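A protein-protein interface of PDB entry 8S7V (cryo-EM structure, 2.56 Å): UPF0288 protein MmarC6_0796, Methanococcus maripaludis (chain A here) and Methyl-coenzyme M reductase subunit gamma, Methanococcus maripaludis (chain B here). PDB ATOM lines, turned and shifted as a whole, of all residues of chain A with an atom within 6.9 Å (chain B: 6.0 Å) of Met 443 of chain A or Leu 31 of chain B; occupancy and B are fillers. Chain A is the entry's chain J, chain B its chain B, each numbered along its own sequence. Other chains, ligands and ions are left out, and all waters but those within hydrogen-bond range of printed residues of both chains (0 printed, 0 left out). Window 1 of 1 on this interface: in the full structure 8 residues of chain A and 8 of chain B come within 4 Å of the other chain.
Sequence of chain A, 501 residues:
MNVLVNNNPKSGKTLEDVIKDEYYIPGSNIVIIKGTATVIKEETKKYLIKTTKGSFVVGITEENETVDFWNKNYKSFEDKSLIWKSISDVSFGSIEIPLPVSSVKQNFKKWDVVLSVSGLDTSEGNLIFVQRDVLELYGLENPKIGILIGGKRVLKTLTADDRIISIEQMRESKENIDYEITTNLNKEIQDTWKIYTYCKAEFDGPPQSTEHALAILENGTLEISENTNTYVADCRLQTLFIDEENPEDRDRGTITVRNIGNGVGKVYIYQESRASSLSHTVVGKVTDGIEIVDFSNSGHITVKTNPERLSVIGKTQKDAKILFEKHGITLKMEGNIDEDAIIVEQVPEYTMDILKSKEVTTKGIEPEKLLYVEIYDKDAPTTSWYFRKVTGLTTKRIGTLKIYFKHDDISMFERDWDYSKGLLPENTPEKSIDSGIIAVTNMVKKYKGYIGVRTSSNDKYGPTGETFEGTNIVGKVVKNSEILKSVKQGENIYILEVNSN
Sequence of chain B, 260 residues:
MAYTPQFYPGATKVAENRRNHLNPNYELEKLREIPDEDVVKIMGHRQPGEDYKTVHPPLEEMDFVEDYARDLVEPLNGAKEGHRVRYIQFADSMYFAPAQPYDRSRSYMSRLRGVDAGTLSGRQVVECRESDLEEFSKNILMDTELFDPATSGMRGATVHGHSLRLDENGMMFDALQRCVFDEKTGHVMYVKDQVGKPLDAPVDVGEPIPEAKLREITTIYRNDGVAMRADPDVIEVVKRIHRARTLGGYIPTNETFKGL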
ATOM      1  N   SER A 420      17.898  35.582 -21.754  1.00  0.00           N
ATOM      2  CA  SER A 420      18.525  34.369 -21.234  1.00  0.00           C
ATOM      3  C   SER A 420      18.511  34.404 -19.706  1.00  0.00           C
ATOM      4  O   SER A 420      19.529  34.595 -19.040  1.00  0.00           O
ATOM      5  CB  SER A 420      19.940  34.233 -21.779  1.00  0.00           C
ATOM      6  OG  SER A 420      20.656  35.448 -21.641  1.00  0.00           O
ATOM      7  N   LYS A 421      17.316  34.214 -19.151  1.00  0.00           N
ATOM      8  CA  LYS A 421      17.123  34.232 -17.708  1.00  0.00           C
ATOM      9  C   LYS A 421      16.711  32.870 -17.164  1.00  0.00           C
ATOM     10  O   LYS A 421      17.390  32.317 -16.296  1.00  0.00           O
ATOM     11  CB  LYS A 421      16.084  35.296 -17.335  1.00  0.00           C
ATOM     12  CG  LYS A 421      16.342  36.656 -17.958  1.00  0.00           C
ATOM     13  CD  LYS A 421      17.727  37.177 -17.606  1.00  0.00           C
ATOM     14  CE  LYS A 421      17.722  37.883 -16.262  1.00  0.00           C
ATOM     15  NZ  LYS A 421      17.659  39.361 -16.417  1.00  0.00           N
ATOM     16  N   GLY A 422      15.619  32.302 -17.661  1.00  0.00           N
ATOM     17  CA  GLY A 422      15.152  31.029 -17.152  1.00  0.00           C
ATOM     18  C   GLY A 422      15.666  29.849 -17.945  1.00  0.00           C
ATOM     19  O   GLY A 422      14.935  28.879 -18.166  1.00  0.00           O
ATOM     20  N   LEU A 423      16.926  29.912 -18.375  1.00  0.00           N
ATOM     21  CA  LEU A 423      17.496  28.885 -19.247  1.00  0.00           C
ATOM     22  C   LEU A 423      17.928  27.676 -18.416  1.00  0.00           C
ATOM     23  O   LEU A 423      19.100  27.304 -18.348  1.00  0.00           O
ATOM     24  CB  LEU A 423      18.658  29.449 -20.051  1.00  0.00           C
ATOM     25  CG  LEU A 423      18.301  30.238 -21.308  1.00  0.00           C
ATOM     26  CD1 LEU A 423      19.562  30.689 -22.018  1.00  0.00           C
ATOM     27  CD2 LEU A 423      17.424  29.418 -22.234  1.00  0.00           C
ATOM     28  N   LEU A 424      16.943  27.052 -17.779  1.00  0.00           N
ATOM     29  CA  LEU A 424      17.192  25.809 -17.073  1.00  0.00           C
ATOM     30  C   LEU A 424      17.570  24.715 -18.069  1.00  0.00           C
ATOM     31  O   LEU A 424      17.130  24.739 -19.221  1.00  0.00           O
ATOM     32  CB  LEU A 424      15.955  25.383 -16.287  1.00  0.00           C
ATOM     33  CG  LEU A 424      15.569  26.194 -15.051  1.00  0.00           C
ATOM     34  CD1 LEU A 424      14.423  25.518 -14.325  1.00  0.00           C
ATOM     35  CD2 LEU A 424      16.757  26.363 -14.125  1.00  0.00           C
ATOM     36  N   PRO A 425      18.397  23.753 -17.658  1.00  0.00           N
ATOM     37  CA  PRO A 425      18.708  22.628 -18.549  1.00  0.00           C
ATOM     38  C   PRO A 425      17.448  21.892 -18.973  1.00  0.00           C
ATOM     39  O   PRO A 425      16.777  21.273 -18.142  1.00  0.00           O
ATOM     40  CB  PRO A 425      19.622  21.743 -17.694  1.00  0.00           C
ATOM     41  CG  PRO A 425      20.206  22.665 -16.684  1.00  0.00           C
ATOM     42  CD  PRO A 425      19.160  23.696 -16.400  1.00  0.00           C
ATOM     43  N   THR A 441      23.588  27.055 -24.720  1.00  0.00           N
ATOM     44  CA  THR A 441      24.165  26.711 -23.429  1.00  0.00           C
ATOM     45  C   THR A 441      23.281  27.267 -22.319  1.00  0.00           C
ATOM     46  O   THR A 441      22.910  28.444 -22.345  1.00  0.00           O
ATOM     47  CB  THR A 441      25.584  27.263 -23.298  1.00  0.00           C
ATOM     48  OG1 THR A 441      25.537  28.560 -22.698  1.00  0.00           O
ATOM     49  CG2 THR A 441      26.227  27.386 -24.660  1.00  0.00           C
ATOM     50  N   ASN A 442      22.946  26.419 -21.352  1.00  0.00           N
ATOM     51  CA  ASN A 442      22.043  26.805 -20.276  1.00  0.00           C
ATOM     52  C   ASN A 442      22.809  27.589 -19.210  1.00  0.00           C
ATOM     53  O   ASN A 442      23.983  27.931 -19.375  1.00  0.00           O
ATOM     54  CB  ASN A 442      21.354  25.573 -19.700  1.00  0.00           C
ATOM     55  CG  ASN A 442      22.299  24.410 -19.514  1.00  0.00           C
ATOM     56  OD1 ASN A 442      23.413  24.579 -19.027  1.00  0.00           O
ATOM     57  ND2 ASN A 442      21.855  23.220 -19.890  1.00  0.00           N
ATOM     58  N   MET A 443      22.147  27.873 -18.089  1.00  0.00           N
ATOM     59  CA  MET A 443      22.731  28.677 -17.024  1.00  0.00           C
ATOM     60  C   MET A 443      23.840  27.956 -16.273  1.00  0.00           C
ATOM     61  O   MET A 443      24.515  28.583 -15.451  1.00  0.00           O
ATOM     62  CB  MET A 443      21.649  29.102 -16.029  1.00  0.00           C
ATOM     63  CG  MET A 443      20.612  28.030 -15.757  1.00  0.00           C
ATOM     64  SD  MET A 443      19.971  28.075 -14.075  1.00  0.00           S
ATOM     65  CE  MET A 443      18.899  29.505 -14.161  1.00  0.00           C
ATOM     66  N   VAL A 444      24.031  26.661 -16.524  1.00  0.00           N
ATOM     67  CA  VAL A 444      25.080  25.912 -15.838  1.00  0.00           C
ATOM     68  C   VAL A 444      26.452  26.466 -16.194  1.00  0.00           C
ATOM     69  O   VAL A 444      27.310  26.657 -15.325  1.00  0.00           O
ATOM     70  CB  VAL A 444      24.976  24.417 -16.180  1.00  0.00           C
ATOM     71  CG1 VAL A 444      26.015  23.635 -15.418  1.00  0.00           C
ATOM     72  CG2 VAL A 444      23.585  23.907 -15.870  1.00  0.00           C
ATOM     73  N   LYS A 445      26.679  26.732 -17.474  1.00  0.00           N
ATOM     74  CA  LYS A 445      27.975  27.196 -17.936  1.00  0.00           C
ATOM     75  C   LYS A 445      28.090  28.710 -17.796  1.00  0.00           C
ATOM     76  O   LYS A 445      27.105  29.420 -17.589  1.00  0.00           O
ATOM     77  CB  LYS A 445      28.205  26.778 -19.387  1.00  0.00           C
ATOM     78  CG  LYS A 445      28.127  25.280 -19.600  1.00  0.00           C
ATOM     79  CD  LYS A 445      29.121  24.553 -18.712  1.00  0.00           C
ATOM     80  CE  LYS A 445      29.117  23.062 -18.985  1.00  0.00           C
ATOM     81  NZ  LYS A 445      29.438  22.276 -17.764  1.00  0.00           N
ATOM     82  N   LYS A 446      29.326  29.198 -17.908  1.00  0.00           N
ATOM     83  CA  LYS A 446      29.573  30.628 -17.756  1.00  0.00           C
ATOM     84  C   LYS A 446      29.017  31.414 -18.936  1.00  0.00           C
ATOM     85  O   LYS A 446      28.520  32.534 -18.765  1.00  0.00           O
ATOM     86  CB  LYS A 446      31.071  30.878 -17.590  1.00  0.00           C
ATOM     87  CG  LYS A 446      31.486  32.337 -17.663  1.00  0.00           C
ATOM     88  CD  LYS A 446      32.994  32.472 -17.562  1.00  0.00           C
ATOM     89  CE  LYS A 446      33.415  32.906 -16.171  1.00  0.00           C
ATOM     90  NZ  LYS A 446      34.600  32.141 -15.693  1.00  0.00           N
ATOM     91  N   TYR A 447      29.087  30.848 -20.139  1.00  0.00           N
ATOM     92  CA  TYR A 447      28.586  31.515 -21.340  1.00  0.00           C
ATOM     93  C   TYR A 447      27.172  31.023 -21.648  1.00  0.00           C
ATOM     94  O   TYR A 447      26.905  30.328 -22.628  1.00  0.00           O
ATOM     95  CB  TYR A 447      29.539  31.289 -22.505  1.00  0.00           C
ATOM     96  CG  TYR A 447      30.916  31.828 -22.221  1.00  0.00           C
ATOM     97  CD1 TYR A 447      31.147  33.194 -22.188  1.00  0.00           C
ATOM     98  CD2 TYR A 447      31.978  30.975 -21.962  1.00  0.00           C
ATOM     99  CE1 TYR A 447      32.395  33.698 -21.918  1.00  0.00           C
ATOM    100  CE2 TYR A 447      33.235  31.473 -21.689  1.00  0.00           C
ATOM    101  CZ  TYR A 447      33.435  32.835 -21.670  1.00  0.00           C
ATOM    102  OH  TYR A 447      34.680  33.346 -21.400  1.00  0.00           O
ATOM    103  N   LYS A 448      26.253  31.416 -20.769  1.00  0.00           N
ATOM    104  CA  LYS A 448      24.855  31.040 -20.904  1.00  0.00           C
ATOM    105  C   LYS A 448      24.189  31.885 -21.980  1.00  0.00           C
ATOM    106  O   LYS A 448      24.366  33.106 -22.021  1.00  0.00           O
ATOM    107  CB  LYS A 448      24.133  31.203 -19.567  1.00  0.00           C
ATOM    108  CG  LYS A 448      22.637  31.430 -19.682  1.00  0.00           C
ATOM    109  CD  LYS A 448      22.087  32.122 -18.449  1.00  0.00           C
ATOM    110  CE  LYS A 448      22.773  33.453 -18.219  1.00  0.00           C
ATOM    111  NZ  LYS A 448      22.186  34.196 -17.073  1.00  0.00           N
ATOM    112  N   GLY A 449      23.429  31.233 -22.856  1.00  0.00           N
ATOM    113  CA  GLY A 449      22.655  31.903 -23.877  1.00  0.00           C
ATOM    114  C   GLY A 449      23.291  31.914 -25.251  1.00  0.00           C
ATOM    115  O   GLY A 449      22.589  32.174 -26.236  1.00  0.00           O
ATOM    116  N   GLY A 470      25.739  21.067 -19.893  1.00  0.00           N
ATOM    117  CA  GLY A 470      25.610  22.498 -20.055  1.00  0.00           C
ATOM    118  C   GLY A 470      25.028  22.944 -21.376  1.00  0.00           C
ATOM    119  O   GLY A 470      25.140  24.128 -21.718  1.00  0.00           O
ATOM    120  N   ASN A 472      21.548  22.572 -24.057  1.00  0.00           N
ATOM    121  CA  ASN A 472      20.202  22.104 -24.353  1.00  0.00           C
ATOM    122  C   ASN A 472      19.899  22.307 -25.831  1.00  0.00           C
ATOM    123  O   ASN A 472      20.048  23.412 -26.361  1.00  0.00           O
ATOM    124  CB  ASN A 472      19.143  22.804 -23.490  1.00  0.00           C
ATOM    125  CG  ASN A 472      19.431  24.271 -23.277  1.00  0.00           C
ATOM    126  OD1 ASN A 472      19.301  24.781 -22.165  1.00  0.00           O
ATOM    127  ND2 ASN A 472      19.804  24.963 -24.343  1.00  0.00           N
ATOM    128  N   GLU B  29      21.293  17.193 -10.284  1.00  0.00           N
ATOM    129  CA  GLU B  29      21.394  18.078 -11.435  1.00  0.00           C
ATOM    130  C   GLU B  29      22.136  19.349 -11.048  1.00  0.00           C
ATOM    131  O   GLU B  29      21.777  20.019 -10.075  1.00  0.00           O
ATOM    132  CB  GLU B  29      20.004  18.414 -11.966  1.00  0.00           C
ATOM    133  CG  GLU B  29      19.957  19.659 -12.832  1.00  0.00           C
ATOM    134  CD  GLU B  29      18.620  19.838 -13.518  1.00  0.00           C
ATOM    135  OE1 GLU B  29      18.326  19.072 -14.459  1.00  0.00           O
ATOM    136  OE2 GLU B  29      17.862  20.745 -13.117  1.00  0.00           O
ATOM    137  N   LYS B  30      23.171  19.682 -11.809  1.00  0.00           N
ATOM    138  CA  LYS B  30      23.942  20.884 -11.543  1.00  0.00           C
ATOM    139  C   LYS B  30      23.338  22.069 -12.287  1.00  0.00           C
ATOM    140  O   LYS B  30      22.895  21.952 -13.431  1.00  0.00           O
ATOM    141  CB  LYS B  30      25.411  20.686 -11.927  1.00  0.00           C
ATOM    142  CG  LYS B  30      25.700  20.670 -13.412  1.00  0.00           C
ATOM    143  CD  LYS B  30      27.198  20.709 -13.669  1.00  0.00           C
ATOM    144  CE  LYS B  30      27.862  21.845 -12.911  1.00  0.00           C
ATOM    145  NZ  LYS B  30      29.053  22.375 -13.627  1.00  0.00           N
ATOM    146  N   LEU B  31      23.299  23.213 -11.604  1.00  0.00           N
ATOM    147  CA  LEU B  31      22.637  24.398 -12.123  1.00  0.00           C
ATOM    148  C   LEU B  31      23.549  25.610 -12.224  1.00  0.00           C
ATOM    149  O   LEU B  31      23.091  26.671 -12.658  1.00  0.00           O
ATOM    150  CB  LEU B  31      21.423  24.752 -11.253  1.00  0.00           C
ATOM    151  CG  LEU B  31      20.354  23.667 -11.123  1.00  0.00           C
ATOM    152  CD1 LEU B  31      19.383  24.003 -10.008  1.00  0.00           C
ATOM    153  CD2 LEU B  31      19.617  23.489 -12.435  1.00  0.00           C
ATOM    154  N   ARG B  32      24.814  25.492 -11.832  1.00  0.00           N
ATOM    155  CA  ARG B  32      25.748  26.601 -11.932  1.00  0.00           C
ATOM    156  C   ARG B  32      27.159  26.042 -11.968  1.00  0.00           C
ATOM    157  O   ARG B  32      27.381  24.850 -11.748  1.00  0.00           O
ATOM    158  CB  ARG B  32      25.588  27.586 -10.769  1.00  0.00           C
ATOM    159  CG  ARG B  32      25.795  26.966  -9.402  1.00  0.00           C
ATOM    160  CD  ARG B  32      25.152  27.807  -8.317  1.00  0.00           C
ATOM    161  NE  ARG B  32      23.702  27.831  -8.443  1.00  0.00           N
ATOM    162  CZ  ARG B  32      22.893  26.897  -7.964  1.00  0.00           C
ATOM    163  NH1 ARG B  32      23.361  25.847  -7.310  1.00  0.00           N
ATOM    164  NH2 ARG B  32      21.582  27.020  -8.143  1.00  0.00           N
ATOM    165  N   GLU B  33      28.113  26.923 -12.255  1.00  0.00           N
ATOM    166  CA  GLU B  33      29.529  26.577 -12.272  1.00  0.00           C
ATOM    167  C   GLU B  33      30.286  27.653 -11.507  1.00  0.00           C
ATOM    168  O   GLU B  33      30.525  28.744 -12.033  1.00  0.00           O
ATOM    169  CB  GLU B  33      30.049  26.448 -13.702  1.00  0.00           C
ATOM    170  CG  GLU B  33      31.544  26.218 -13.800  1.00  0.00           C
ATOM    171  CD  GLU B  33      31.947  24.833 -13.335  1.00  0.00           C
ATOM    172  OE1 GLU B  33      31.132  23.899 -13.478  1.00  0.00           O
ATOM    173  OE2 GLU B  33      33.080  24.678 -12.829  1.00  0.00           O
ATOM    174  N   ASP B 143      27.350  23.553  -6.569  1.00  0.00           N
ATOM    175  CA  ASP B 143      27.066  23.524  -7.996  1.00  0.00           C
ATOM    176  C   ASP B 143      25.774  22.805  -8.352  1.00  0.00           C
ATOM    177  O   ASP B 143      25.295  22.961  -9.479  1.00  0.00           O
ATOM    178  CB  ASP B 143      28.225  22.869  -8.757  1.00  0.00           C
ATOM    179  CG  ASP B 143      29.420  23.786  -8.905  1.00  0.00           C
ATOM    180  OD1 ASP B 143      29.437  24.854  -8.259  1.00  0.00           O
ATOM    181  OD2 ASP B 143      30.342  23.440  -9.671  1.00  0.00           O
ATOM    182  N   THR B 144      25.193  22.040  -7.436  1.00  0.00           N
ATOM    183  CA  THR B 144      24.048  21.208  -7.766  1.00  0.00           C
ATOM    184  C   THR B 144      22.752  21.900  -7.348  1.00  0.00           C
ATOM    185  O   THR B 144      22.741  23.059  -6.928  1.00  0.00           O
ATOM    186  CB  THR B 144      24.183  19.835  -7.115  1.00  0.00           C
ATOM    187  OG1 THR B 144      24.347  19.991  -5.701  1.00  0.00           O
ATOM    188  CG2 THR B 144      25.384  19.100  -7.678  1.00  0.00           C
ATOM    189  N   GLU B 145      21.638  21.180  -7.465  1.00  0.00           N
ATOM    190  CA  GLU B 145      20.324  21.692  -7.105  1.00  0.00           C
ATOM    191  C   GLU B 145      20.132  21.830  -5.603  1.00  0.00           C
ATOM    192  O   GLU B 145      19.123  22.401  -5.178  1.00  0.00           O
ATOM    193  CB  GLU B 145      19.237  20.783  -7.677  1.00  0.00           C
ATOM    194  CG  GLU B 145      19.292  19.364  -7.148  1.00  0.00           C
ATOM    195  CD  GLU B 145      18.445  18.411  -7.959  1.00  0.00           C
ATOM    196  OE1 GLU B 145      17.712  18.880  -8.854  1.00  0.00           O
ATOM    197  OE2 GLU B 145      18.510  17.191  -7.704  1.00  0.00           O
ATOM    198  N   PHE B 147      21.600  23.803  -3.756  1.00  0.00           N
ATOM    199  CA  PHE B 147      21.851  25.192  -3.406  1.00  0.00           C
ATOM    200  C   PHE B 147      21.068  26.113  -4.328  1.00  0.00           C
ATOM    201  O   PHE B 147      21.086  25.948  -5.551  1.00  0.00           O
ATOM    202  CB  PHE B 147      23.345  25.516  -3.497  1.00  0.00           C
ATOM    203  CG  PHE B 147      23.674  26.952  -3.212  1.00  0.00           C
ATOM    204  CD1 PHE B 147      23.486  27.484  -1.950  1.00  0.00           C
ATOM    205  CD2 PHE B 147      24.175  27.769  -4.209  1.00  0.00           C
ATOM    206  CE1 PHE B 147      23.790  28.804  -1.689  1.00  0.00           C
ATOM    207  CE2 PHE B 147      24.479  29.090  -3.954  1.00  0.00           C
ATOM    208  CZ  PHE B 147      24.287  29.607  -2.692  1.00  0.00           C
ATOM    209  N   GLU B 207      22.191  32.809 -10.813  1.00  0.00           N
ATOM    210  CA  GLU B 207      20.954  33.545 -10.637  1.00  0.00           C
ATOM    211  C   GLU B 207      19.944  32.716  -9.859  1.00  0.00           C
ATOM    212  O   GLU B 207      20.023  31.484  -9.835  1.00  0.00           O
ATOM    213  CB  GLU B 207      20.379  33.940 -11.999  1.00  0.00           C
ATOM    214  CG  GLU B 207      19.563  32.870 -12.677  1.00  0.00           C
ATOM    215  CD  GLU B 207      18.898  33.384 -13.931  1.00  0.00           C
ATOM    216  OE1 GLU B 207      19.589  33.500 -14.965  1.00  0.00           O
ATOM    217  OE2 GLU B 207      17.688  33.685 -13.880  1.00  0.00           O
ATOM    218  N   PRO B 208      18.995  33.365  -9.184  1.00  0.00           N
ATOM    219  CA  PRO B 208      18.020  32.615  -8.383  1.00  0.00           C
ATOM    220  C   PRO B 208      17.226  31.630  -9.227  1.00  0.00           C
ATOM    221  O   PRO B 208      16.864  31.911 -10.371  1.00  0.00           O
ATOM    222  CB  PRO B 208      17.114  33.708  -7.802  1.00  0.00           C
ATOM    223  CG  PRO B 208      17.523  34.988  -8.443  1.00  0.00           C
ATOM    224  CD  PRO B 208      18.900  34.816  -8.965  1.00  0.00           C
ATOM    225  N   ILE B 209      16.964  30.467  -8.646  1.00  0.00           N
ATOM    226  CA  ILE B 209      16.158  29.440  -9.317  1.00  0.00           C
ATOM    227  C   ILE B 209      14.725  29.940  -9.448  1.00  0.00           C
ATOM    228  O   ILE B 209      14.183  30.508  -8.484  1.00  0.00           O
ATOM    229  CB  ILE B 209      16.216  28.127  -8.532  1.00  0.00           C
ATOM    230  CG1 ILE B 209      17.667  27.682  -8.345  1.00  0.00           C
ATOM    231  CG2 ILE B 209      15.426  27.043  -9.233  1.00  0.00           C
ATOM    232  CD1 ILE B 209      18.433  27.552  -9.638  1.00  0.00           C
ATOM    233  N   PRO B 210      14.080  29.775 -10.602  1.00  0.00           N
ATOM    234  CA  PRO B 210      12.682  30.201 -10.730  1.00  0.00           C
ATOM    235  C   PRO B 210      11.787  29.458  -9.749  1.00  0.00           C
ATOM    236  O   PRO B 210      12.016  28.291  -9.424  1.00  0.00           O
ATOM    237  CB  PRO B 210      12.333  29.855 -12.181  1.00  0.00           C
ATOM    238  CG  PRO B 210      13.646  29.800 -12.883  1.00  0.00           C
ATOM    239  CD  PRO B 210      14.625  29.284 -11.879  1.00  0.00           C
ATOM    240  N   LYS B 213      10.432  25.976 -10.580  1.00  0.00           N
ATOM    241  CA  LYS B 213      11.383  24.897 -10.339  1.00  0.00           C
ATOM    242  C   LYS B 213      11.567  24.641  -8.849  1.00  0.00           C
ATOM    243  O   LYS B 213      11.762  23.490  -8.435  1.00  0.00           O
ATOM    244  CB  LYS B 213      12.720  25.230 -10.999  1.00  0.00           C
ATOM    245  CG  LYS B 213      13.808  24.195 -10.789  1.00  0.00           C
ATOM    246  CD  LYS B 213      13.591  22.982 -11.668  1.00  0.00           C
ATOM    247  CE  LYS B 213      14.869  22.180 -11.817  1.00  0.00           C
ATOM    248  NZ  LYS B 213      14.700  21.048 -12.767  1.00  0.00           N
ATOM    249  N   ILE B 217      11.583  21.047  -6.812  1.00  0.00           N
ATOM    250  CA  ILE B 217      12.802  20.480  -6.243  1.00  0.00           C
ATOM    251  C   ILE B 217      12.906  20.675  -4.737  1.00  0.00           C
ATOM    252  O   ILE B 217      13.911  20.264  -4.140  1.00  0.00           O
ATOM    253  CB  ILE B 217      14.058  21.049  -6.933  1.00  0.00           C
ATOM    254  CG1 ILE B 217      14.253  22.521  -6.565  1.00  0.00           C
ATOM    255  CG2 ILE B 217      13.962  20.873  -8.437  1.00  0.00           C
ATOM    256  CD1 ILE B 217      15.516  23.120  -7.131  1.00  0.00           C
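Of chain B, only Leu 31 and Glu 207 come within 4 Å of Met 443 of chain A.
Of the printed residues of chain A, Leu 31 of chain B touches Pro 425, Met 443 and Val 444.
Of the printed residues of chain B, Lys 448 of chain A touches Glu 207.
Printed residues of chain A within 4 Å of Lys 213 of chain B: Leu 424 (3.7 Å).
Of the printed residues of chain B, Leu 424 of chain A touches Lys 213.
Printed residues of chain A within 4 Å of Glu 33 of chain B: Val 444 (3.2 Å).
The nearest residue of chain B that does not touch Met 443 of chain A is Arg 32 of chain B (4.2 Å).
Among the printed residues, merely in contact across the chains: Val 444 of chain A with Lys 30 of chain B (3.2 Å), Val 444 of chain A with Arg 32 of chain B (3.4 Å), Met 443 of chain A with Glu 207 of chain B (3.7 Å), Leu 424 of chain A with Lys 213 of chain B (3.7 Å), Val 444 of chain A with Leu 31 of chain B (3.8 Å) and Pro 425 of chain A with Leu 31 of chain B (3.997 Å).
O of Val 444 of chain A lies within hydrogen-bond range of N of Glu 33 of chain B (3.2 Å).
The side-chain amino group (NZ) of Lys 448 of chain A is in salt-bridge range of the side-chain carboxylate (OE1) of Glu 207 of chain B (3.4 Å).
O of Lys 421 of chain A lies close to OE2 of Glu 207 of chain B, at 2.8 Å.
SD of Met 443 of chain A sits close to O of Leu 31 of chain B (3.7 Å).
The side-chain carboxylate (OE2) of Glu 29 of chain B is in salt-bridge range of the side-chain amino group (NZ) of Lys 213 of chain B, 3.2 Å away.
The backbone NH of Leu 31 of chain B sits at hydrogen-bond distance from the backbone carbonyl oxygen of Asp 143 of chain B, 2.9 Å away.
O of Thr 144 of chain B is in hydrogen-bond range of NH1 of Arg 32 of chain B (2.9 Å).
The backbone carbonyl oxygen (O) of Ser 420 of chain A is in hydrogen-bond range of the side-chain amino group (NZ) of Lys 448 of chain A (3.3 Å).
O of Leu 423 of chain A sits close to N of Met 443 of chain A (3.1 Å).
OD1 of Asn 442 of chain A lies close to N of Val 444 of chain A.
Printed residues of chain B that touch a printed residue of chain A: Lys 30, Leu 31, Arg 32, Glu 33, Glu 207 and Lys 213.
Hydrophobic or aromatic side chains of chain B that line the printed part of chain A: Leu 31.
Of the 17 printed residues of chain A, 6 touch a printed residue of chain B.
Hydrophobic or aromatic side chains of chain A that line the printed part of chain B: Leu 424, Pro 425, Met 443 and Val 444.
Among the printed residues, Asp or Glu carboxylates within 4 Å of a Lys or Arg side-chain nitrogen of the other chain: Lys 448 of chain A with Glu 207 of chain B.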
